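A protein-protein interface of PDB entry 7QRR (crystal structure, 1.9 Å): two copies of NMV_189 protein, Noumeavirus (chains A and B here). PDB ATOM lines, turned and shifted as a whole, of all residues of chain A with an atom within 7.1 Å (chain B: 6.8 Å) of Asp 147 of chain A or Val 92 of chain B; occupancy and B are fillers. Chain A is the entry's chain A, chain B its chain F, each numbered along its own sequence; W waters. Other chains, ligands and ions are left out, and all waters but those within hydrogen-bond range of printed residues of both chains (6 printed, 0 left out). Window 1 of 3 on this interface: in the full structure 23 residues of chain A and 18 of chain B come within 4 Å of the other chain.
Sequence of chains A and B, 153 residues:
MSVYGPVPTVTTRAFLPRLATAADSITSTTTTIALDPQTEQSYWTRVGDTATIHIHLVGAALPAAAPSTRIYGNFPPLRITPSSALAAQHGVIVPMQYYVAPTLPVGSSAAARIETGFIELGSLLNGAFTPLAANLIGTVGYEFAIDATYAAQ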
ATOM      1  N   GLU A  40      -1.480   7.891  25.119  1.00  0.00           N
ATOM      2  CA  GLU A  40      -0.358   8.793  24.943  1.00  0.00           C
ATOM      3  C   GLU A  40      -0.795  10.212  25.270  1.00  0.00           C
ATOM      4  O   GLU A  40      -1.861  10.658  24.839  1.00  0.00           O
ATOM      5  CB  GLU A  40       0.181   8.694  23.512  1.00  0.00           C
ATOM      6  CG  GLU A  40       1.362   9.614  23.207  1.00  0.00           C
ATOM      7  CD  GLU A  40       1.952   9.346  21.827  1.00  0.00           C
ATOM      8  OE1 GLU A  40       2.294   8.180  21.547  1.00  0.00           O
ATOM      9  OE2 GLU A  40       2.077  10.292  21.018  1.00  0.00           O
ATOM     10  N   TYR A  43      -0.266  17.310  24.438  1.00  0.00           N
ATOM     11  CA  TYR A  43       0.202  18.491  25.148  1.00  0.00           C
ATOM     12  C   TYR A  43       0.492  19.620  24.189  1.00  0.00           C
ATOM     13  O   TYR A  43       0.592  19.418  22.972  1.00  0.00           O
ATOM     14  CB  TYR A  43       1.464  18.169  25.974  1.00  0.00           C
ATOM     15  CG  TYR A  43       2.656  17.740  25.120  1.00  0.00           C
ATOM     16  CD1 TYR A  43       3.403  18.679  24.415  1.00  0.00           C
ATOM     17  CD2 TYR A  43       3.016  16.398  25.010  1.00  0.00           C
ATOM     18  CE1 TYR A  43       4.469  18.306  23.619  1.00  0.00           C
ATOM     19  CE2 TYR A  43       4.097  16.009  24.215  1.00  0.00           C
ATOM     20  CZ  TYR A  43       4.815  16.980  23.524  1.00  0.00           C
ATOM     21  OH  TYR A  43       5.883  16.635  22.731  1.00  0.00           O
ATOM     22  N   THR A  52       3.931  25.025  20.175  1.00  0.00           N
ATOM     23  CA  THR A  52       4.183  23.686  19.653  1.00  0.00           C
ATOM     24  C   THR A  52       3.134  22.736  20.203  1.00  0.00           C
ATOM     25  O   THR A  52       2.911  22.690  21.412  1.00  0.00           O
ATOM     26  CB  THR A  52       5.597  23.201  20.015  1.00  0.00           C
ATOM     27  OG1 THR A  52       6.552  24.054  19.378  1.00  0.00           O
ATOM     28  CG2 THR A  52       5.831  21.759  19.543  1.00  0.00           C
ATOM     29  N   ILE A  53       2.457  21.996  19.322  1.00  0.00           N
ATOM     30  CA  ILE A  53       1.438  21.062  19.783  1.00  0.00           C
ATOM     31  C   ILE A  53       1.807  19.605  19.485  1.00  0.00           C
ATOM     32  O   ILE A  53       2.469  19.306  18.488  1.00  0.00           O
ATOM     33  CB  ILE A  53       0.067  21.354  19.143  1.00  0.00           C
ATOM     34  CG1 ILE A  53       0.184  21.283  17.619  1.00  0.00           C
ATOM     35  CG2 ILE A  53      -0.451  22.730  19.563  1.00  0.00           C
ATOM     36  CD1 ILE A  53      -1.157  21.300  16.917  1.00  0.00           C
ATOM     37  N   HIS A  54       1.388  18.717  20.386  1.00  0.00           N
ATOM     38  CA  HIS A  54       1.475  17.278  20.173  1.00  0.00           C
ATOM     39  C   HIS A  54       0.128  16.646  20.487  1.00  0.00           C
ATOM     40  O   HIS A  54      -0.333  16.686  21.623  1.00  0.00           O
ATOM     41  CB  HIS A  54       2.552  16.630  21.043  1.00  0.00           C
ATOM     42  CG  HIS A  54       2.594  15.142  20.909  1.00  0.00           C
ATOM     43  ND1 HIS A  54       3.034  14.513  19.760  1.00  0.00           N
ATOM     44  CD2 HIS A  54       2.211  14.156  21.753  1.00  0.00           C
ATOM     45  CE1 HIS A  54       2.934  13.205  19.914  1.00  0.00           C
ATOM     46  NE2 HIS A  54       2.437  12.962  21.113  1.00  0.00           N
ATOM     47  N   ILE A  55      -0.500  16.060  19.477  1.00  0.00           N
ATOM     48  CA  ILE A  55      -1.808  15.436  19.643  1.00  0.00           C
ATOM     49  C   ILE A  55      -1.704  13.975  19.264  1.00  0.00           C
ATOM     50  O   ILE A  55      -1.123  13.656  18.230  1.00  0.00           O
ATOM     51  CB  ILE A  55      -2.880  16.120  18.761  1.00  0.00           C
ATOM     52  CG1 ILE A  55      -3.133  17.550  19.234  1.00  0.00           C
ATOM     53  CG2 ILE A  55      -4.179  15.309  18.740  1.00  0.00           C
ATOM     54  CD1 ILE A  55      -3.793  18.423  18.185  1.00  0.00           C
ATOM     55  N   VAL A  94       0.028  21.105   7.762  1.00  0.00           N
ATOM     56  CA  VAL A  94       1.138  20.298   8.246  1.00  0.00           C
ATOM     57  C   VAL A  94       0.928  18.819   7.897  1.00  0.00           C
ATOM     58  O   VAL A  94      -0.206  18.384   7.699  1.00  0.00           O
ATOM     59  CB  VAL A  94       1.307  20.442   9.784  1.00  0.00           C
ATOM     60  CG1 VAL A  94       1.648  21.889  10.155  1.00  0.00           C
ATOM     61  CG2 VAL A  94       0.047  19.978  10.501  1.00  0.00           C
ATOM     62  N   PRO A  95       2.021  18.037   7.826  1.00  0.00           N
ATOM     63  CA  PRO A  95       1.812  16.590   7.682  1.00  0.00           C
ATOM     64  C   PRO A  95       1.244  16.014   8.978  1.00  0.00           C
ATOM     65  O   PRO A  95       1.264  16.701  10.012  1.00  0.00           O
ATOM     66  CB  PRO A  95       3.225  16.057   7.429  1.00  0.00           C
ATOM     67  CG  PRO A  95       4.117  17.019   8.211  1.00  0.00           C
ATOM     68  CD  PRO A  95       3.449  18.383   7.986  1.00  0.00           C
ATOM     69  N   MET A  96       0.757  14.782   8.948  1.00  0.00           N
ATOM     70  CA  MET A  96       0.427  14.107  10.198  1.00  0.00           C
ATOM     71  C   MET A  96       0.720  12.621  10.062  1.00  0.00           C
ATOM     72  O   MET A  96       0.994  12.138   8.971  1.00  0.00           O
ATOM     73  CB  MET A  96      -1.034  14.347  10.605  1.00  0.00           C
ATOM     74  CG  MET A  96      -2.088  13.822   9.625  1.00  0.00           C
ATOM     75  SD  MET A  96      -3.774  14.054  10.267  1.00  0.00           S
ATOM     76  CE  MET A  96      -3.814  12.797  11.556  1.00  0.00           C
ATOM     77  N   GLN A  97       0.669  11.917  11.187  1.00  0.00           N
ATOM     78  CA  GLN A  97       1.084  10.528  11.246  1.00  0.00           C
ATOM     79  C   GLN A  97      -0.102   9.614  11.524  1.00  0.00           C
ATOM     80  O   GLN A  97      -0.950   9.929  12.355  1.00  0.00           O
ATOM     81  CB  GLN A  97       2.167  10.348  12.322  1.00  0.00           C
ATOM     82  CG  GLN A  97       2.660   8.906  12.445  1.00  0.00           C
ATOM     83  CD  GLN A  97       3.728   8.744  13.498  1.00  0.00           C
ATOM     84  OE1 GLN A  97       3.980   9.654  14.307  1.00  0.00           O
ATOM     85  NE2 GLN A  97       4.374   7.590  13.495  1.00  0.00           N
ATOM     86  N   TYR A  99      -0.949   5.636  12.669  1.00  0.00           N
ATOM     87  CA  TYR A  99      -0.532   4.306  13.116  1.00  0.00           C
ATOM     88  C   TYR A  99      -1.462   3.194  12.621  1.00  0.00           C
ATOM     89  O   TYR A  99      -1.085   2.024  12.579  1.00  0.00           O
ATOM     90  CB  TYR A  99      -0.469   4.260  14.641  1.00  0.00           C
ATOM     91  CG  TYR A  99       0.592   5.151  15.241  1.00  0.00           C
ATOM     92  CD1 TYR A  99       1.880   4.675  15.455  1.00  0.00           C
ATOM     93  CD2 TYR A  99       0.305   6.464  15.597  1.00  0.00           C
ATOM     94  CE1 TYR A  99       2.860   5.480  16.018  1.00  0.00           C
ATOM     95  CE2 TYR A  99       1.281   7.287  16.160  1.00  0.00           C
ATOM     96  CZ  TYR A  99       2.555   6.784  16.369  1.00  0.00           C
ATOM     97  OH  TYR A  99       3.531   7.572  16.935  1.00  0.00           O
ATOM     98  N   ALA A 112      -2.925  17.860   8.053  1.00  0.00           N
ATOM     99  CA  ALA A 112      -3.880  18.512   8.939  1.00  0.00           C
ATOM    100  C   ALA A 112      -3.881  20.000   8.639  1.00  0.00           C
ATOM    101  O   ALA A 112      -2.841  20.561   8.292  1.00  0.00           O
ATOM    102  CB  ALA A 112      -3.525  18.251  10.417  1.00  0.00           C
ATOM    103  N   ILE A 114      -4.403  23.457  10.391  1.00  0.00           N
ATOM    104  CA  ILE A 114      -4.514  24.130  11.679  1.00  0.00           C
ATOM    105  C   ILE A 114      -5.181  25.483  11.461  1.00  0.00           C
ATOM    106  O   ILE A 114      -4.698  26.308  10.680  1.00  0.00           O
ATOM    107  CB  ILE A 114      -3.141  24.304  12.343  1.00  0.00           C
ATOM    108  CG1 ILE A 114      -2.492  22.933  12.527  1.00  0.00           C
ATOM    109  CG2 ILE A 114      -3.286  24.995  13.726  1.00  0.00           C
ATOM    110  CD1 ILE A 114      -1.049  23.003  12.987  1.00  0.00           C
ATOM    111  N   ALA A 145      -1.427  10.900  15.026  1.00  0.00           N
ATOM    112  CA  ALA A 145      -0.768  11.962  15.781  1.00  0.00           C
ATOM    113  C   ALA A 145      -0.574  13.198  14.915  1.00  0.00           C
ATOM    114  O   ALA A 145      -0.363  13.096  13.706  1.00  0.00           O
ATOM    115  CB  ALA A 145       0.575  11.490  16.323  1.00  0.00           C
ATOM    116  N   ILE A 146      -0.653  14.368  15.539  1.00  0.00           N
ATOM    117  CA  ILE A 146      -0.413  15.620  14.841  1.00  0.00           C
ATOM    118  C   ILE A 146       0.625  16.417  15.613  1.00  0.00           C
ATOM    119  O   ILE A 146       0.470  16.654  16.814  1.00  0.00           O
ATOM    120  CB  ILE A 146      -1.698  16.460  14.679  1.00  0.00           C
ATOM    121  CG1 ILE A 146      -2.778  15.660  13.932  1.00  0.00           C
ATOM    122  CG2 ILE A 146      -1.375  17.763  13.947  1.00  0.00           C
ATOM    123  CD1 ILE A 146      -4.167  16.305  14.006  1.00  0.00           C
ATOM    124  N   ASP A 147       1.686  16.805  14.920  1.00  0.00           N
ATOM    125  CA  ASP A 147       2.792  17.560  15.504  1.00  0.00           C
ATOM    126  C   ASP A 147       3.047  18.829  14.693  1.00  0.00           C
ATOM    127  O   ASP A 147       3.176  18.765  13.475  1.00  0.00           O
ATOM    128  CB  ASP A 147       4.049  16.691  15.555  1.00  0.00           C
ATOM    129  CG  ASP A 147       3.907  15.547  16.534  1.00  0.00           C
ATOM    130  OD1 ASP A 147       3.914  15.834  17.747  1.00  0.00           O
ATOM    131  OD2 ASP A 147       3.776  14.372  16.104  1.00  0.00           O
ATOM    132  N   ALA A 148       3.108  19.983  15.356  1.00  0.00           N
ATOM    133  CA  ALA A 148       3.266  21.244  14.636  1.00  0.00           C
ATOM    134  C   ALA A 148       3.748  22.372  15.531  1.00  0.00           C
ATOM    135  O   ALA A 148       3.604  22.311  16.746  1.00  0.00           O
ATOM    136  CB  ALA A 148       1.961  21.649  13.992  1.00  0.00           C
ATOM    137  N   THR A 149       4.296  23.398  14.897  1.00  0.00           N
ATOM    138  CA  THR A 149       4.708  24.620  15.573  1.00  0.00           C
ATOM    139  C   THR A 149       4.203  25.787  14.740  1.00  0.00           C
ATOM    140  O   THR A 149       4.365  25.799  13.518  1.00  0.00           O
ATOM    141  CB  THR A 149       6.242  24.697  15.742  1.00  0.00           C
ATOM    142  OG1 THR A 149       6.712  23.560  16.482  1.00  0.00           O
ATOM    143  CG2 THR A 149       6.666  25.996  16.442  1.00  0.00           C
ATOM    144  N   LEU B  78      13.120  14.351  22.977  1.00  0.00           N
ATOM    145  CA  LEU B  78      11.699  14.538  22.690  1.00  0.00           C
ATOM    146  C   LEU B  78      10.799  14.225  23.891  1.00  0.00           C
ATOM    147  O   LEU B  78      10.946  13.194  24.552  1.00  0.00           O
ATOM    148  CB  LEU B  78      11.283  13.657  21.506  1.00  0.00           C
ATOM    149  CG  LEU B  78       9.780  13.585  21.230  1.00  0.00           C
ATOM    150  CD1 LEU B  78       9.243  14.932  20.737  1.00  0.00           C
ATOM    151  CD2 LEU B  78       9.496  12.481  20.226  1.00  0.00           C
ATOM    152  N   ARG B  79       9.866  15.130  24.167  1.00  0.00           N
ATOM    153  CA  ARG B  79       8.820  14.853  25.141  1.00  0.00           C
ATOM    154  C   ARG B  79       7.728  13.998  24.513  1.00  0.00           C
ATOM    155  O   ARG B  79       6.977  14.484  23.665  1.00  0.00           O
ATOM    156  CB  ARG B  79       8.217  16.160  25.665  1.00  0.00           C
ATOM    157  CG  ARG B  79       7.062  15.923  26.627  1.00  0.00           C
ATOM    158  CD  ARG B  79       6.401  17.220  27.061  1.00  0.00           C
ATOM    159  NE  ARG B  79       5.235  16.934  27.897  1.00  0.00           N
ATOM    160  CZ  ARG B  79       4.979  17.536  29.055  1.00  0.00           C
ATOM    161  NH1 ARG B  79       5.810  18.468  29.517  1.00  0.00           N
ATOM    162  NH2 ARG B  79       3.896  17.200  29.748  1.00  0.00           N
ATOM    163  N   ILE B  80       7.635  12.730  24.912  1.00  0.00           N
ATOM    164  CA  ILE B  80       6.539  11.871  24.467  1.00  0.00           C
ATOM    165  C   ILE B  80       6.371  10.690  25.414  1.00  0.00           C
ATOM    166  O   ILE B  80       7.350  10.183  25.965  1.00  0.00           O
ATOM    167  CB  ILE B  80       6.762  11.363  23.012  1.00  0.00           C
ATOM    168  CG1 ILE B  80       5.471  10.760  22.437  1.00  0.00           C
ATOM    169  CG2 ILE B  80       7.936  10.389  22.936  1.00  0.00           C
ATOM    170  CD1 ILE B  80       5.501  10.610  20.920  1.00  0.00           C
ATOM    171  N   GLN B  89       9.556   2.817  19.357  1.00  0.00           N
ATOM    172  CA  GLN B  89       8.967   3.856  20.188  1.00  0.00           C
ATOM    173  C   GLN B  89       8.218   4.856  19.313  1.00  0.00           C
ATOM    174  O   GLN B  89       8.666   5.161  18.210  1.00  0.00           O
ATOM    175  CB  GLN B  89      10.056   4.568  20.998  1.00  0.00           C
ATOM    176  CG  GLN B  89      10.597   3.734  22.147  1.00  0.00           C
ATOM    177  CD  GLN B  89       9.522   3.432  23.163  1.00  0.00           C
ATOM    178  OE1 GLN B  89       9.043   4.332  23.854  1.00  0.00           O
ATOM    179  NE2 GLN B  89       9.118   2.169  23.249  1.00  0.00           N
ATOM    180  N   HIS B  90       7.080   5.350  19.797  1.00  0.00           N
ATOM    181  CA  HIS B  90       6.372   6.422  19.102  1.00  0.00           C
ATOM    182  C   HIS B  90       7.263   7.643  19.016  1.00  0.00           C
ATOM    183  O   HIS B  90       7.988   7.966  19.962  1.00  0.00           O
ATOM    184  CB  HIS B  90       5.068   6.782  19.814  1.00  0.00           C
ATOM    185  CG  HIS B  90       3.972   5.783  19.611  1.00  0.00           C
ATOM    186  ND1 HIS B  90       2.655   6.056  19.911  1.00  0.00           N
ATOM    187  CD2 HIS B  90       3.994   4.514  19.141  1.00  0.00           C
ATOM    188  CE1 HIS B  90       1.914   4.997  19.644  1.00  0.00           C
ATOM    189  NE2 HIS B  90       2.701   4.049  19.167  1.00  0.00           N
ATOM    190  N   GLY B  91       7.214   8.322  17.879  1.00  0.00           N
ATOM    191  CA  GLY B  91       7.993   9.527  17.701  1.00  0.00           C
ATOM    192  C   GLY B  91       7.294  10.546  16.817  1.00  0.00           C
ATOM    193  O   GLY B  91       6.134  10.368  16.431  1.00  0.00           O
ATOM    194  N   VAL B  92       8.003  11.623  16.506  1.00  0.00           N
ATOM    195  CA  VAL B  92       7.475  12.670  15.642  1.00  0.00           C
ATOM    196  C   VAL B  92       8.040  12.463  14.246  1.00  0.00           C
ATOM    197  O   VAL B  92       9.254  12.366  14.078  1.00  0.00           O
ATOM    198  CB  VAL B  92       7.840  14.071  16.155  1.00  0.00           C
ATOM    199  CG1 VAL B  92       7.399  15.143  15.173  1.00  0.00           C
ATOM    200  CG2 VAL B  92       7.235  14.303  17.560  1.00  0.00           C
ATOM    201  N   ILE B  93       7.171  12.384  13.248  1.00  0.00           N
ATOM    202  CA  ILE B  93       7.659  12.188  11.873  1.00  0.00           C
ATOM    203  C   ILE B  93       7.822  13.527  11.171  1.00  0.00           C
ATOM    204  O   ILE B  93       6.889  14.334  11.137  1.00  0.00           O
ATOM    205  CB  ILE B  93       6.702  11.306  11.026  1.00  0.00           C
ATOM    206  CG1 ILE B  93       6.297  10.040  11.796  1.00  0.00           C
ATOM    207  CG2 ILE B  93       7.348  10.983   9.663  1.00  0.00           C
ATOM    208  CD1 ILE B  93       7.466   9.177  12.279  1.00  0.00           C
ATOM    209  N   VAL B  94       8.989  13.746  10.574  1.00  0.00           N
ATOM    210  CA  VAL B  94       9.262  14.976   9.847  1.00  0.00           C
ATOM    211  C   VAL B  94       9.814  14.644   8.468  1.00  0.00           C
ATOM    212  O   VAL B  94      10.317  13.541   8.260  1.00  0.00           O
ATOM    213  CB  VAL B  94      10.267  15.854  10.612  1.00  0.00           C
ATOM    214  CG1 VAL B  94       9.717  16.204  12.004  1.00  0.00           C
ATOM    215  CG2 VAL B  94      11.603  15.128  10.736  1.00  0.00           C
ATOM    216  N   ALA B 112      12.088  11.409   8.549  1.00  0.00           N
ATOM    217  CA  ALA B 112      12.824  10.933   9.717  1.00  0.00           C
ATOM    218  C   ALA B 112      11.858  10.766  10.887  1.00  0.00           C
ATOM    219  O   ALA B 112      10.867  11.487  10.982  1.00  0.00           O
ATOM    220  CB  ALA B 112      13.964  11.891  10.075  1.00  0.00           C
ATOM    221  N   ARG B 113      12.138   9.805  11.766  1.00  0.00           N
ATOM    222  CA  ARG B 113      11.328   9.610  12.971  1.00  0.00           C
ATOM    223  C   ARG B 113      12.135  10.070  14.167  1.00  0.00           C
ATOM    224  O   ARG B 113      13.158   9.474  14.490  1.00  0.00           O
ATOM    225  CB  ARG B 113      10.914   8.137  13.138  1.00  0.00           C
ATOM    226  CG  ARG B 113      10.299   7.794  14.517  1.00  0.00           C
ATOM    227  CD  ARG B 113       9.549   6.450  14.537  1.00  0.00           C
ATOM    228  NE  ARG B 113      10.335   5.307  14.039  1.00  0.00           N
ATOM    229  CZ  ARG B 113       9.786   4.162  13.637  1.00  0.00           C
ATOM    230  NH1 ARG B 113       8.461   4.015  13.681  1.00  0.00           N
ATOM    231  NH2 ARG B 113      10.540   3.165  13.179  1.00  0.00           N
ATOM    232  N   ILE B 114      11.684  11.143  14.801  1.00  0.00           N
ATOM    233  CA  ILE B 114      12.357  11.667  15.971  1.00  0.00           C
ATOM    234  C   ILE B 114      11.792  10.990  17.200  1.00  0.00           C
ATOM    235  O   ILE B 114      10.594  11.078  17.462  1.00  0.00           O
ATOM    236  CB  ILE B 114      12.185  13.200  16.081  1.00  0.00           C
ATOM    237  CG1 ILE B 114      12.806  13.866  14.852  1.00  0.00           C
ATOM    238  CG2 ILE B 114      12.819  13.726  17.343  1.00  0.00           C
ATOM    239  CD1 ILE B 114      12.375  15.278  14.685  1.00  0.00           C
ATOM    240  N   GLU B 115      12.666  10.306  17.936  1.00  0.00           N
ATOM    241  CA  GLU B 115      12.317   9.662  19.192  1.00  0.00           C
ATOM    242  C   GLU B 115      13.126  10.288  20.327  1.00  0.00           C
ATOM    243  O   GLU B 115      14.097  11.003  20.085  1.00  0.00           O
ATOM    244  CB  GLU B 115      12.574   8.146  19.118  1.00  0.00           C
ATOM    245  CG  GLU B 115      11.866   7.452  17.939  1.00  0.00           C
ATOM    246  CD  GLU B 115      12.228   5.982  17.781  1.00  0.00           C
ATOM    247  OE1 GLU B 115      12.743   5.373  18.753  1.00  0.00           O
ATOM    248  OE2 GLU B 115      11.988   5.432  16.674  1.00  0.00           O
ATOM    249  N   PHE B 129       5.237   5.754   8.762  1.00  0.00           N
ATOM    250  CA  PHE B 129       6.698   5.811   8.671  1.00  0.00           C
ATOM    251  C   PHE B 129       7.291   4.412   8.523  1.00  0.00           C
ATOM    252  O   PHE B 129       6.926   3.505   9.272  1.00  0.00           O
ATOM    253  CB  PHE B 129       7.292   6.492   9.909  1.00  0.00           C
ATOM    254  CG  PHE B 129       8.795   6.551   9.903  1.00  0.00           C
ATOM    255  CD1 PHE B 129       9.459   7.600   9.272  1.00  0.00           C
ATOM    256  CD2 PHE B 129       9.548   5.559  10.535  1.00  0.00           C
ATOM    257  CE1 PHE B 129      10.849   7.659   9.272  1.00  0.00           C
ATOM    258  CE2 PHE B 129      10.934   5.602  10.522  1.00  0.00           C
ATOM    259  CZ  PHE B 129      11.583   6.656   9.896  1.00  0.00           C
ATOM    260  N   ALA B 148      13.993  20.096  12.204  1.00  0.00           N
ATOM    261  CA  ALA B 148      12.760  19.862  12.949  1.00  0.00           C
ATOM    262  C   ALA B 148      12.650  20.739  14.189  1.00  0.00           C
ATOM    263  O   ALA B 148      13.660  21.214  14.715  1.00  0.00           O
ATOM    264  CB  ALA B 148      12.663  18.401  13.342  1.00  0.00           C
ATOM    265  N   THR B 149      11.414  20.951  14.633  1.00  0.00           N
ATOM    266  CA  THR B 149      11.137  21.616  15.904  1.00  0.00           C
ATOM    267  C   THR B 149      10.143  20.770  16.694  1.00  0.00           C
ATOM    268  O   THR B 149       9.134  20.323  16.147  1.00  0.00           O
ATOM    269  CB  THR B 149      10.580  23.051  15.696  1.00  0.00           C
ATOM    270  OG1 THR B 149      11.549  23.838  14.987  1.00  0.00           O
ATOM    271  CG2 THR B 149      10.264  23.715  17.047  1.00  0.00           C
ATOM    272  N   TYR B 150      10.432  20.543  17.975  1.00  0.00           N
ATOM    273  CA  TYR B 150       9.619  19.663  18.804  1.00  0.00           C
ATOM    274  C   TYR B 150       9.769  20.081  20.264  1.00  0.00           C
ATOM    275  O   TYR B 150      10.698  20.813  20.596  1.00  0.00           O
ATOM    276  CB  TYR B 150      10.033  18.193  18.613  1.00  0.00           C
ATOM    277  CG  TYR B 150      11.485  17.922  18.935  1.00  0.00           C
ATOM    278  CD1 TYR B 150      11.884  17.585  20.231  1.00  0.00           C
ATOM    279  CD2 TYR B 150      12.460  18.013  17.954  1.00  0.00           C
ATOM    280  CE1 TYR B 150      13.211  17.344  20.537  1.00  0.00           C
ATOM    281  CE2 TYR B 150      13.797  17.782  18.251  1.00  0.00           C
ATOM    282  CZ  TYR B 150      14.167  17.451  19.546  1.00  0.00           C
ATOM    283  OH  TYR B 150      15.498  17.221  19.836  1.00  0.00           O
ATOM    284  N   ALA B 151       8.859  19.624  21.119  1.00  0.00           N
ATOM    285  CA  ALA B 151       8.938  19.916  22.551  1.00  0.00           C
ATOM    286  C   ALA B 151       9.841  18.914  23.259  1.00  0.00           C
ATOM    287  O   ALA B 151       9.793  17.716  22.981  1.00  0.00           O
ATOM    288  CB  ALA B 151       7.554  19.909  23.177  1.00  0.00           C
HETATM  289  O   HOH W   1       6.075   7.139  15.502  1.00  0.00           O
HETATM  290  O   HOH W   2       4.038   5.561  11.444  1.00  0.00           O
HETATM  291  O   HOH W   3       4.241  12.660  13.913  1.00  0.00           O
HETATM  292  O   HOH W   4       7.171  21.549  14.732  1.00  0.00           O
HETATM  293  O   HOH W   5       3.881  11.874  17.336  1.00  0.00           O
HETATM  294  O   HOH W   6       6.832  17.851  20.332  1.00  0.00           O
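The side-chain amide oxygen of Gln 97 of chain A sits close to the backbone carbonyl oxygen of Gly 91 of chain B, at 3.1 Å. The side-chain hydroxyl (OH) of Tyr 99 of chain A lies close to a ring nitrogen (ND1) of His 90 of chain B (3.5 Å). The backbone carbonyl oxygen (O) of Arg 79 of chain B lies within hydrogen-bond range of the side-chain hydroxyl (OH) of Tyr 43 of chain A. A ring nitrogen (ND1) of His 90 of chain B is in hydrogen-bond range of the side-chain carboxylate (OE1) of Glu 40 of chain A, at 2.7 Å.
The backbone carbonyl oxygen (O) of Gln 97 of chain A is in hydrogen-bond range of the backbone NH (N) of Ala 145 of chain A. The backbone NH of Arg 79 of chain B sits at hydrogen-bond distance from the backbone carbonyl oxygen of Ala 151 of chain B, at 2.8 Å. OE2 of Glu 40 of chain A lies within hydrogen-bond range of NE2 of His 54 of chain A, 2.7 Å away. A ring nitrogen (ND1) of His 54 of chain A sits at hydrogen-bond distance from the side-chain carboxylate of Asp 147 of chain A (2.6 Å). The side-chain hydroxyl of Thr 52 of chain A sits at hydrogen-bond distance from the side-chain hydroxyl of Thr 149 of chain A. The backbone carbonyl oxygen of Tyr 43 of chain A sits at hydrogen-bond distance from the backbone NH of His 54 of chain A, 2.8 Å away.
OE2 of Glu 40 of chain A touches CD1 of Ile 80 of chain B (3.4 Å). Tyr 43 of chain A touches Ala 151 of chain B. Ile 80 of chain B touches His 54 of chain A (CD1 to CE1, 3.8 Å). Gln 97 of chain A touches Ile 93 of chain B (CD to CG1, 3.3 Å). OH of Tyr 99 of chain A touches O of Gly 91 of chain B (3.9 Å). Asp 147 of chain A touches Val 92 of chain B. Thr 149 of chain A touches Thr 149 of chain B (OG1 to CG2, 3.6 Å).
Of the printed residues of chain B, His 54 of chain A touches Ile 80 (3.8 Å). Ile 55 of chain A touches none of the printed residues of chain B. Pro 95 of chain A touches none of the printed residues of chain B. Of the printed residues of chain B, Gln 97 of chain A touches Gly 91 (3.1 Å) and Ile 93 (3.3 Å). Asp 147 of chain A touches one residue of chain B. Printed residues of chain B within 4 Å of Thr 149 of chain A: Thr 149. Of the printed residues of chain A, His 90 of chain B touches Glu 40 and Tyr 99. Of the printed residues of chain A, Val 92 of chain B touches Asp 147. Of the printed residues of chain A, Ile 93 of chain B touches Gln 97 (3.3 Å). The nearest residue of chain B that does not touch Asp 147 of chain A is Gly 91 of chain B (4.7 Å).
Printed residues of chain A that touch a printed residue of chain B: Glu 40, Tyr 43, His 54, Gln 97, Tyr 99, Asp 147 and Thr 149. Hydrophobic or aromatic side chains of chain A that line the printed part of chain B: Tyr 43, His 54 and Tyr 99. Among the printed residues, no Asp or Glu carboxylate lies within 4 Å of a Lys or Arg side-chain nitrogen of the other chain.
Thr 149 of chain B touches its own counterpart, Thr 149 of chain A. Positions printed for both chains: 94, 112, 114, 148 and 149. Of the 11 pairs that touch across the chains among the printed residues, 1 has its exchanged pair printed and touching as well.
Water W1 lies within hydrogen-bond range of NE2 of Gln 97 of chain A (2.7 Å), N of Gly 91 of chain B (2.9 Å) and OH of Tyr 99 of chain A (3.0 Å). Water W4 bridges the side-chain hydroxyl (OG1) of Thr 149 of chain A (2.7 Å) and the backbone carbonyl oxygen (O) of Thr 149 of chain B (2.7 Å). Water W5 lies within hydrogen-bond range of OD2 of Asp 147 of chain A and O of Gly 91 of chain B. Water W6 lies within hydrogen-bond range of N of Ala 151 of chain B (2.8 Å) and OH of Tyr 43 of chain A (2.9 Å). Water W3 lies within hydrogen-bond range of the side-chain carboxylate (OD2) of Asp 147 of chain A (2.8 Å), the backbone NH (N) of Ile 93 of chain B (3.0 Å) and the side-chain amide oxygen (OE1) of Gln 97 of chain A (3.0 Å).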
